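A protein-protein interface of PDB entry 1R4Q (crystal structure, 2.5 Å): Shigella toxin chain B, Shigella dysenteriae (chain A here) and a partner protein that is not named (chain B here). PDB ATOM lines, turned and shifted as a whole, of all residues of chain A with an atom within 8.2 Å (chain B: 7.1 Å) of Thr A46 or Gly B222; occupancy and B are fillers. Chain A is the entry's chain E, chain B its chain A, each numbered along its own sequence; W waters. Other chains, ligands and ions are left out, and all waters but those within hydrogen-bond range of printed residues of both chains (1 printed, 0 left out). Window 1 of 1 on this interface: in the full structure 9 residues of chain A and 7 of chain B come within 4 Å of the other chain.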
ATOM      1  N   LYS A   8      16.582  27.295  18.387  1.00  0.00           N
ATOM      2  CA  LYS A   8      15.889  27.524  19.648  1.00  0.00           C
ATOM      3  C   LYS A   8      14.374  27.606  19.350  1.00  0.00           C
ATOM      4  O   LYS A   8      13.977  27.913  18.229  1.00  0.00           O
ATOM      5  CB  LYS A   8      16.374  28.837  20.273  1.00  0.00           C
ATOM      6  CG  LYS A   8      17.848  28.850  20.625  1.00  0.00           C
ATOM      7  CD  LYS A   8      18.282  30.139  21.312  1.00  0.00           C
ATOM      8  CE  LYS A   8      19.799  30.260  21.339  1.00  0.00           C
ATOM      9  NZ  LYS A   8      20.221  31.482  22.047  1.00  0.00           N
ATOM     10  N   VAL A   9      13.534  27.305  20.333  1.00  0.00           N
ATOM     11  CA  VAL A   9      12.085  27.383  20.188  1.00  0.00           C
ATOM     12  C   VAL A   9      11.701  28.865  20.391  1.00  0.00           C
ATOM     13  O   VAL A   9      12.008  29.426  21.465  1.00  0.00           O
ATOM     14  CB  VAL A   9      11.450  26.578  21.321  1.00  0.00           C
ATOM     15  CG1 VAL A   9       9.927  26.476  21.142  1.00  0.00           C
ATOM     16  CG2 VAL A   9      12.129  25.224  21.418  1.00  0.00           C
ATOM     17  N   LEU A  39       8.505  19.161  27.938  1.00  0.00           N
ATOM     18  CA  LEU A  39       9.888  19.155  27.531  1.00  0.00           C
ATOM     19  C   LEU A  39      10.142  20.287  26.538  1.00  0.00           C
ATOM     20  O   LEU A  39      11.158  21.000  26.656  1.00  0.00           O
ATOM     21  CB  LEU A  39      10.304  17.802  26.933  1.00  0.00           C
ATOM     22  CG  LEU A  39      10.179  16.538  27.811  1.00  0.00           C
ATOM     23  CD1 LEU A  39      10.739  15.323  27.072  1.00  0.00           C
ATOM     24  CD2 LEU A  39      10.884  16.726  29.113  1.00  0.00           C
ATOM     25  N   LEU A  40       9.259  20.494  25.561  1.00  0.00           N
ATOM     26  CA  LEU A  40       9.504  21.606  24.634  1.00  0.00           C
ATOM     27  C   LEU A  40       9.353  22.937  25.333  1.00  0.00           C
ATOM     28  O   LEU A  40      10.119  23.842  25.094  1.00  0.00           O
ATOM     29  CB  LEU A  40       8.602  21.518  23.423  1.00  0.00           C
ATOM     30  CG  LEU A  40       9.027  20.290  22.588  1.00  0.00           C
ATOM     31  CD1 LEU A  40       8.011  20.120  21.487  1.00  0.00           C
ATOM     32  CD2 LEU A  40      10.431  20.452  21.968  1.00  0.00           C
ATOM     33  N   LEU A  41       8.387  23.059  26.237  1.00  0.00           N
ATOM     34  CA  LEU A  41       8.217  24.300  26.978  1.00  0.00           C
ATOM     35  C   LEU A  41       9.505  24.613  27.728  1.00  0.00           C
ATOM     36  O   LEU A  41       9.937  25.757  27.740  1.00  0.00           O
ATOM     37  CB  LEU A  41       7.068  24.195  27.968  1.00  0.00           C
ATOM     38  CG  LEU A  41       6.834  25.516  28.701  1.00  0.00           C
ATOM     39  CD1 LEU A  41       6.484  26.623  27.760  1.00  0.00           C
ATOM     40  CD2 LEU A  41       5.775  25.295  29.709  1.00  0.00           C
ATOM     41  N   SER A  42      10.121  23.607  28.350  1.00  0.00           N
ATOM     42  CA  SER A  42      11.377  23.800  29.104  1.00  0.00           C
ATOM     43  C   SER A  42      12.536  24.156  28.158  1.00  0.00           C
ATOM     44  O   SER A  42      13.450  24.901  28.509  1.00  0.00           O
ATOM     45  CB  SER A  42      11.736  22.528  29.901  1.00  0.00           C
ATOM     46  OG  SER A  42      10.787  22.267  30.918  1.00  0.00           O
ATOM     47  N   ALA A  43      12.484  23.605  26.955  1.00  0.00           N
ATOM     48  CA  ALA A  43      13.500  23.875  25.958  1.00  0.00           C
ATOM     49  C   ALA A  43      13.395  25.354  25.588  1.00  0.00           C
ATOM     50  O   ALA A  43      14.365  26.015  25.198  1.00  0.00           O
ATOM     51  CB  ALA A  43      13.253  23.002  24.768  1.00  0.00           C
ATOM     52  N   GLN A  44      12.189  25.875  25.709  1.00  0.00           N
ATOM     53  CA  GLN A  44      11.976  27.269  25.427  1.00  0.00           C
ATOM     54  C   GLN A  44      12.404  28.132  26.643  1.00  0.00           C
ATOM     55  O   GLN A  44      13.065  29.169  26.481  1.00  0.00           O
ATOM     56  CB  GLN A  44      10.517  27.499  25.069  1.00  0.00           C
ATOM     57  CG  GLN A  44      10.143  28.935  25.143  1.00  0.00           C
ATOM     58  CD  GLN A  44       8.760  29.207  24.620  1.00  0.00           C
ATOM     59  OE1 GLN A  44       7.949  28.315  24.501  1.00  0.00           O
ATOM     60  NE2 GLN A  44       8.490  30.450  24.303  1.00  0.00           N
ATOM     61  N   ILE A  45      12.065  27.710  27.860  1.00  0.00           N
ATOM     62  CA  ILE A  45      12.438  28.508  29.020  1.00  0.00           C
ATOM     63  C   ILE A  45      13.947  28.690  29.198  1.00  0.00           C
ATOM     64  O   ILE A  45      14.390  29.750  29.667  1.00  0.00           O
ATOM     65  CB  ILE A  45      11.820  27.923  30.333  1.00  0.00           C
ATOM     66  CG1 ILE A  45      10.349  28.292  30.394  1.00  0.00           C
ATOM     67  CG2 ILE A  45      12.527  28.466  31.574  1.00  0.00           C
ATOM     68  CD1 ILE A  45       9.580  27.321  31.192  1.00  0.00           C
ATOM     69  N   THR A  46      14.715  27.677  28.798  1.00  0.00           N
ATOM     70  CA  THR A  46      16.195  27.637  28.935  1.00  0.00           C
ATOM     71  C   THR A  46      17.007  27.935  27.649  1.00  0.00           C
ATOM     72  O   THR A  46      18.223  27.942  27.687  1.00  0.00           O
ATOM     73  CB  THR A  46      16.673  26.247  29.483  1.00  0.00           C
ATOM     74  OG1 THR A  46      16.305  25.233  28.560  1.00  0.00           O
ATOM     75  CG2 THR A  46      16.015  25.882  30.772  1.00  0.00           C
ATOM     76  N   GLY A  47      16.357  28.150  26.511  1.00  0.00           N
ATOM     77  CA  GLY A  47      17.084  28.479  25.288  1.00  0.00           C
ATOM     78  C   GLY A  47      17.838  27.349  24.629  1.00  0.00           C
ATOM     79  O   GLY A  47      18.727  27.565  23.811  1.00  0.00           O
ATOM     80  N   MET A  48      17.459  26.133  24.990  1.00  0.00           N
ATOM     81  CA  MET A  48      18.063  24.911  24.495  1.00  0.00           C
ATOM     82  C   MET A  48      17.895  24.813  22.989  1.00  0.00           C
ATOM     83  O   MET A  48      16.931  25.343  22.448  1.00  0.00           O
ATOM     84  CB  MET A  48      17.418  23.744  25.247  1.00  0.00           C
ATOM     85  CG  MET A  48      17.993  22.407  24.902  1.00  0.00           C
ATOM     86  SD  MET A  48      17.336  21.105  25.962  1.00  0.00           S
ATOM     87  CE  MET A  48      17.456  22.074  27.502  1.00  0.00           C
ATOM     88  N   THR A  49      18.844  24.182  22.295  1.00  0.00           N
ATOM     89  CA  THR A  49      18.738  24.042  20.827  1.00  0.00           C
ATOM     90  C   THR A  49      18.197  22.647  20.509  1.00  0.00           C
ATOM     91  O   THR A  49      18.624  21.648  21.101  1.00  0.00           O
ATOM     92  CB  THR A  49      20.121  24.205  20.086  1.00  0.00           C
ATOM     93  OG1 THR A  49      20.662  25.517  20.306  1.00  0.00           O
ATOM     94  CG2 THR A  49      19.957  23.996  18.597  1.00  0.00           C
ATOM     95  N   ARG A  69      19.547  19.213  22.184  1.00  0.00           N
ATOM     96  CA  ARG A  69      20.989  19.344  22.118  1.00  0.00           C
ATOM     97  C   ARG A  69      21.604  20.208  23.180  1.00  0.00           C
ATOM     98  O   ARG A  69      20.892  20.580  24.122  1.00  0.00           O
ATOM     99  CB  ARG A  69      21.375  19.894  20.761  1.00  0.00           C
ATOM    100  CG  ARG A  69      20.822  19.125  19.655  1.00  0.00           C
ATOM    101  CD  ARG A  69      21.388  19.648  18.405  1.00  0.00           C
ATOM    102  NE  ARG A  69      20.817  18.997  17.239  1.00  0.00           N
ATOM    103  CZ  ARG A  69      21.120  17.780  16.853  1.00  0.00           C
ATOM    104  NH1 ARG A  69      22.003  17.076  17.535  1.00  0.00           N
ATOM    105  NH2 ARG A  69      20.508  17.266  15.808  1.00  0.00           N
ATOM    106  OXT ARG A  69      22.804  20.510  23.034  1.00  0.00           O
ATOM    107  N   ASN B 202      16.260  39.831  30.737  1.00  0.00           N
ATOM    108  CA  ASN B 202      16.680  39.146  31.959  1.00  0.00           C
ATOM    109  C   ASN B 202      17.623  39.959  32.885  1.00  0.00           C
ATOM    110  O   ASN B 202      18.360  39.392  33.712  1.00  0.00           O
ATOM    111  CB  ASN B 202      17.318  37.797  31.577  1.00  0.00           C
ATOM    112  CG  ASN B 202      16.292  36.747  31.177  1.00  0.00           C
ATOM    113  OD1 ASN B 202      15.611  36.200  32.042  1.00  0.00           O
ATOM    114  ND2 ASN B 202      16.171  36.455  29.867  1.00  0.00           N
ATOM    115  N   ARG B 205      16.669  39.518  36.841  1.00  0.00           N
ATOM    116  CA  ARG B 205      17.036  38.193  37.312  1.00  0.00           C
ATOM    117  C   ARG B 205      18.547  37.973  37.320  1.00  0.00           C
ATOM    118  O   ARG B 205      19.081  37.374  38.261  1.00  0.00           O
ATOM    119  CB  ARG B 205      16.315  37.100  36.522  1.00  0.00           C
ATOM    120  CG  ARG B 205      14.945  36.773  37.124  1.00  0.00           C
ATOM    121  CD  ARG B 205      14.335  35.474  36.637  1.00  0.00           C
ATOM    122  NE  ARG B 205      14.125  35.500  35.192  1.00  0.00           N
ATOM    123  CZ  ARG B 205      13.705  34.453  34.467  1.00  0.00           C
ATOM    124  NH1 ARG B 205      13.436  33.269  35.046  1.00  0.00           N
ATOM    125  NH2 ARG B 205      13.563  34.577  33.141  1.00  0.00           N
ATOM    126  N   ARG B 220      23.376  30.028  34.469  1.00  0.00           N
ATOM    127  CA  ARG B 220      22.204  29.927  33.614  1.00  0.00           C
ATOM    128  C   ARG B 220      20.985  30.642  34.215  1.00  0.00           C
ATOM    129  O   ARG B 220      20.563  30.345  35.332  1.00  0.00           O
ATOM    130  CB  ARG B 220      21.863  28.451  33.346  1.00  0.00           C
ATOM    131  CG  ARG B 220      23.054  27.490  33.324  1.00  0.00           C
ATOM    132  CD  ARG B 220      23.361  26.833  31.976  1.00  0.00           C
ATOM    133  NE  ARG B 220      22.335  25.926  31.422  1.00  0.00           N
ATOM    134  CZ  ARG B 220      21.218  26.285  30.742  1.00  0.00           C
ATOM    135  NH1 ARG B 220      20.891  27.568  30.493  1.00  0.00           N
ATOM    136  NH2 ARG B 220      20.422  25.331  30.265  1.00  0.00           N
ATOM    137  N   VAL B 221      20.427  31.587  33.466  1.00  0.00           N
ATOM    138  CA  VAL B 221      19.254  32.335  33.899  1.00  0.00           C
ATOM    139  C   VAL B 221      18.316  32.434  32.698  1.00  0.00           C
ATOM    140  O   VAL B 221      18.636  33.096  31.718  1.00  0.00           O
ATOM    141  CB  VAL B 221      19.650  33.777  34.350  1.00  0.00           C
ATOM    142  CG1 VAL B 221      18.428  34.610  34.647  1.00  0.00           C
ATOM    143  CG2 VAL B 221      20.523  33.699  35.571  1.00  0.00           C
ATOM    144  N   GLY B 222      17.171  31.782  32.730  1.00  0.00           N
ATOM    145  CA  GLY B 222      16.326  31.927  31.571  1.00  0.00           C
ATOM    146  C   GLY B 222      16.983  31.367  30.332  1.00  0.00           C
ATOM    147  O   GLY B 222      17.626  30.318  30.349  1.00  0.00           O
ATOM    148  N   ARG B 223      16.818  32.067  29.225  1.00  0.00           N
ATOM    149  CA  ARG B 223      17.376  31.617  27.958  1.00  0.00           C
ATOM    150  C   ARG B 223      18.815  32.039  27.833  1.00  0.00           C
ATOM    151  O   ARG B 223      19.467  31.721  26.839  1.00  0.00           O
ATOM    152  CB  ARG B 223      16.600  32.220  26.786  1.00  0.00           C
ATOM    153  CG  ARG B 223      15.135  31.845  26.733  1.00  0.00           C
ATOM    154  CD  ARG B 223      14.489  32.705  25.711  1.00  0.00           C
ATOM    155  NE  ARG B 223      14.845  32.421  24.327  1.00  0.00           N
ATOM    156  CZ  ARG B 223      14.462  31.326  23.674  1.00  0.00           C
ATOM    157  NH1 ARG B 223      13.742  30.408  24.281  1.00  0.00           N
ATOM    158  NH2 ARG B 223      14.703  31.185  22.394  1.00  0.00           N
ATOM    159  N   ILE B 224      19.314  32.774  28.808  1.00  0.00           N
ATOM    160  CA  ILE B 224      20.690  33.225  28.750  1.00  0.00           C
ATOM    161  C   ILE B 224      21.643  32.207  29.374  1.00  0.00           C
ATOM    162  O   ILE B 224      21.393  31.706  30.476  1.00  0.00           O
ATOM    163  CB  ILE B 224      20.862  34.533  29.508  1.00  0.00           C
ATOM    164  CG1 ILE B 224      20.010  35.638  28.869  1.00  0.00           C
ATOM    165  CG2 ILE B 224      22.352  34.863  29.579  1.00  0.00           C
ATOM    166  CD1 ILE B 224      20.298  35.847  27.426  1.00  0.00           C
ATOM    167  N   SER B 225      22.754  31.898  28.714  1.00  0.00           N
ATOM    168  CA  SER B 225      23.664  30.903  29.312  1.00  0.00           C
ATOM    169  C   SER B 225      25.116  31.287  29.132  1.00  0.00           C
ATOM    170  O   SER B 225      25.545  31.591  28.026  1.00  0.00           O
ATOM    171  CB  SER B 225      23.394  29.552  28.679  1.00  0.00           C
ATOM    172  OG  SER B 225      24.206  28.548  29.230  1.00  0.00           O
ATOM    173  N   TRP B 277      22.365  28.579  38.949  1.00  0.00           N
ATOM    174  CA  TRP B 277      21.011  28.781  38.398  1.00  0.00           C
ATOM    175  C   TRP B 277      20.190  29.867  39.128  1.00  0.00           C
ATOM    176  O   TRP B 277      20.462  30.153  40.289  1.00  0.00           O
ATOM    177  CB  TRP B 277      20.232  27.478  38.538  1.00  0.00           C
ATOM    178  CG  TRP B 277      20.600  26.390  37.576  1.00  0.00           C
ATOM    179  CD1 TRP B 277      21.431  25.319  37.795  1.00  0.00           C
ATOM    180  CD2 TRP B 277      20.074  26.230  36.248  1.00  0.00           C
ATOM    181  NE1 TRP B 277      21.444  24.497  36.683  1.00  0.00           N
ATOM    182  CE2 TRP B 277      20.619  25.029  35.724  1.00  0.00           C
ATOM    183  CE3 TRP B 277      19.185  26.993  35.449  1.00  0.00           C
ATOM    184  CZ2 TRP B 277      20.304  24.565  34.448  1.00  0.00           C
ATOM    185  CZ3 TRP B 277      18.870  26.536  34.181  1.00  0.00           C
ATOM    186  CH2 TRP B 277      19.428  25.324  33.689  1.00  0.00           C
ATOM    187  N   ASP B 278      19.206  30.497  38.477  1.00  0.00           N
ATOM    188  CA  ASP B 278      18.364  31.432  39.227  1.00  0.00           C
ATOM    189  C   ASP B 278      17.277  30.439  39.622  1.00  0.00           C
ATOM    190  O   ASP B 278      16.980  29.525  38.853  1.00  0.00           O
ATOM    191  CB  ASP B 278      17.847  32.571  38.349  1.00  0.00           C
ATOM    192  CG  ASP B 278      16.566  32.241  37.646  1.00  0.00           C
ATOM    193  OD1 ASP B 278      15.477  32.397  38.224  1.00  0.00           O
ATOM    194  OD2 ASP B 278      16.652  31.820  36.485  1.00  0.00           O
ATOM    195  N   THR B 281      13.934  29.800  37.310  1.00  0.00           N
ATOM    196  CA  THR B 281      14.179  28.930  36.169  1.00  0.00           C
ATOM    197  C   THR B 281      14.302  27.500  36.618  1.00  0.00           C
ATOM    198  O   THR B 281      13.694  26.621  36.054  1.00  0.00           O
ATOM    199  CB  THR B 281      15.441  29.286  35.394  1.00  0.00           C
ATOM    200  OG1 THR B 281      15.344  30.631  34.921  1.00  0.00           O
ATOM    201  CG2 THR B 281      15.579  28.366  34.152  1.00  0.00           C
ATOM    202  N   LEU B 282      15.087  27.238  37.637  1.00  0.00           N
ATOM    203  CA  LEU B 282      15.203  25.855  38.080  1.00  0.00           C
ATOM    204  C   LEU B 282      13.855  25.285  38.449  1.00  0.00           C
ATOM    205  O   LEU B 282      13.555  24.154  38.108  1.00  0.00           O
ATOM    206  CB  LEU B 282      16.104  25.725  39.308  1.00  0.00           C
ATOM    207  CG  LEU B 282      17.469  25.084  39.170  1.00  0.00           C
ATOM    208  CD1 LEU B 282      17.813  24.495  40.491  1.00  0.00           C
ATOM    209  CD2 LEU B 282      17.446  24.009  38.133  1.00  0.00           C
ATOM    210  N   ILE B 285      11.400  24.307  35.377  1.00  0.00           N
ATOM    211  CA  ILE B 285      11.702  23.166  34.501  1.00  0.00           C
ATOM    212  C   ILE B 285      11.749  21.802  35.188  1.00  0.00           C
ATOM    213  O   ILE B 285      11.939  20.770  34.526  1.00  0.00           O
ATOM    214  CB  ILE B 285      13.049  23.354  33.746  1.00  0.00           C
ATOM    215  CG1 ILE B 285      14.230  23.245  34.724  1.00  0.00           C
ATOM    216  CG2 ILE B 285      13.051  24.663  32.995  1.00  0.00           C
ATOM    217  CD1 ILE B 285      15.546  23.685  34.114  1.00  0.00           C
HETATM  218  O   HOH W   1      19.265  33.234  24.427  1.00  0.00           O
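The side-chain hydroxyl of Thr B281 sits at hydrogen-bond distance from the guanidinium group of Arg B205 (3.3 Å).
The backbone carbonyl oxygen (O) of Arg B220 sits at hydrogen-bond distance from the backbone NH (N) of Asp B278, at 3.4 Å.
O of Ser A42 sits at hydrogen-bond distance from OG1 of Thr A46 (2.9 Å).
The side-chain hydroxyl (OG1) of Thr B281 is in hydrogen-bond range of the backbone NH (N) of Gly B222 (3.1 Å).
The side-chain carboxylate of Asp B278 lies within hydrogen-bond range of the backbone NH of Thr B281.
Hydrophobic or aromatic side chains of chain B that line the printed part of chain A: Ile B285.
Hydrophobic or aromatic side chains of chain A within 4 Å of the printed part of chain B: Ile A45.
Among the printed residues, 12 pairs touch across the chains.
Among the printed residues, no Asp or Glu carboxylate lies within 4 Å of a Lys or Arg side-chain nitrogen of the other chain.
The guanidinium group of Arg B223 lies within hydrogen-bond range of the backbone carbonyl oxygen of Val A9, at 3.3 Å.
The guanidinium group (NH1) of Arg B223 sits at hydrogen-bond distance from the backbone carbonyl oxygen (O) of Gln A44.
N of Arg B223 sits at hydrogen-bond distance from O of Ile A45 (3.4 Å).
O of Gly B222 sits close to O of Ile A45, at 3.4 Å.
NH2 of Arg B223 touches CB of Lys A8 (3.6 Å).
Ser A42 touches Ile B285.
CG2 of Thr B281 touches CG2 of Ile A45, 3.996 Å away.
Thr A46 touches Arg B220 (O to NH1, 3.9 Å).
Thr A46 touches Gly B222.
Thr A46 touches Arg B223 (C to CA, 3.7 Å).
CG2 of Ile B285 touches CG2 of Thr A46, 3.9 Å away.
Arg B223 touches Gly A47.
Water W1 bridges the backbone carbonyl oxygen of Arg B223 (2.9 Å) and the side-chain amino group of Lys A8 (3.1 Å).
Of the printed residues of chain B, Lys A8 touches Arg B223.
Leu A41 touches none of the printed residues of chain B.
Of the printed residues of chain B, Ser A42 touches Ile B285 (3.8 Å).
Thr A46 touches just these residues of chain B: Arg B220 (3.9 Å), Gly B222 (3.4 Å), Arg B223 (3.7 Å) and Ile B285 (3.9 Å).
Gly B222 touches just these residues of chain A: Ile A45 and Thr A46.
The nearest residue of chain B that does not touch Thr A46 is Thr B281 (4.2 Å).
The nearest residue of chain A that does not touch Gly B222 is Gly A47 (4.6 Å).
The nearest printed residue of chain B that does not touch Gln A44 is Gly B222 (5.9 Å).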
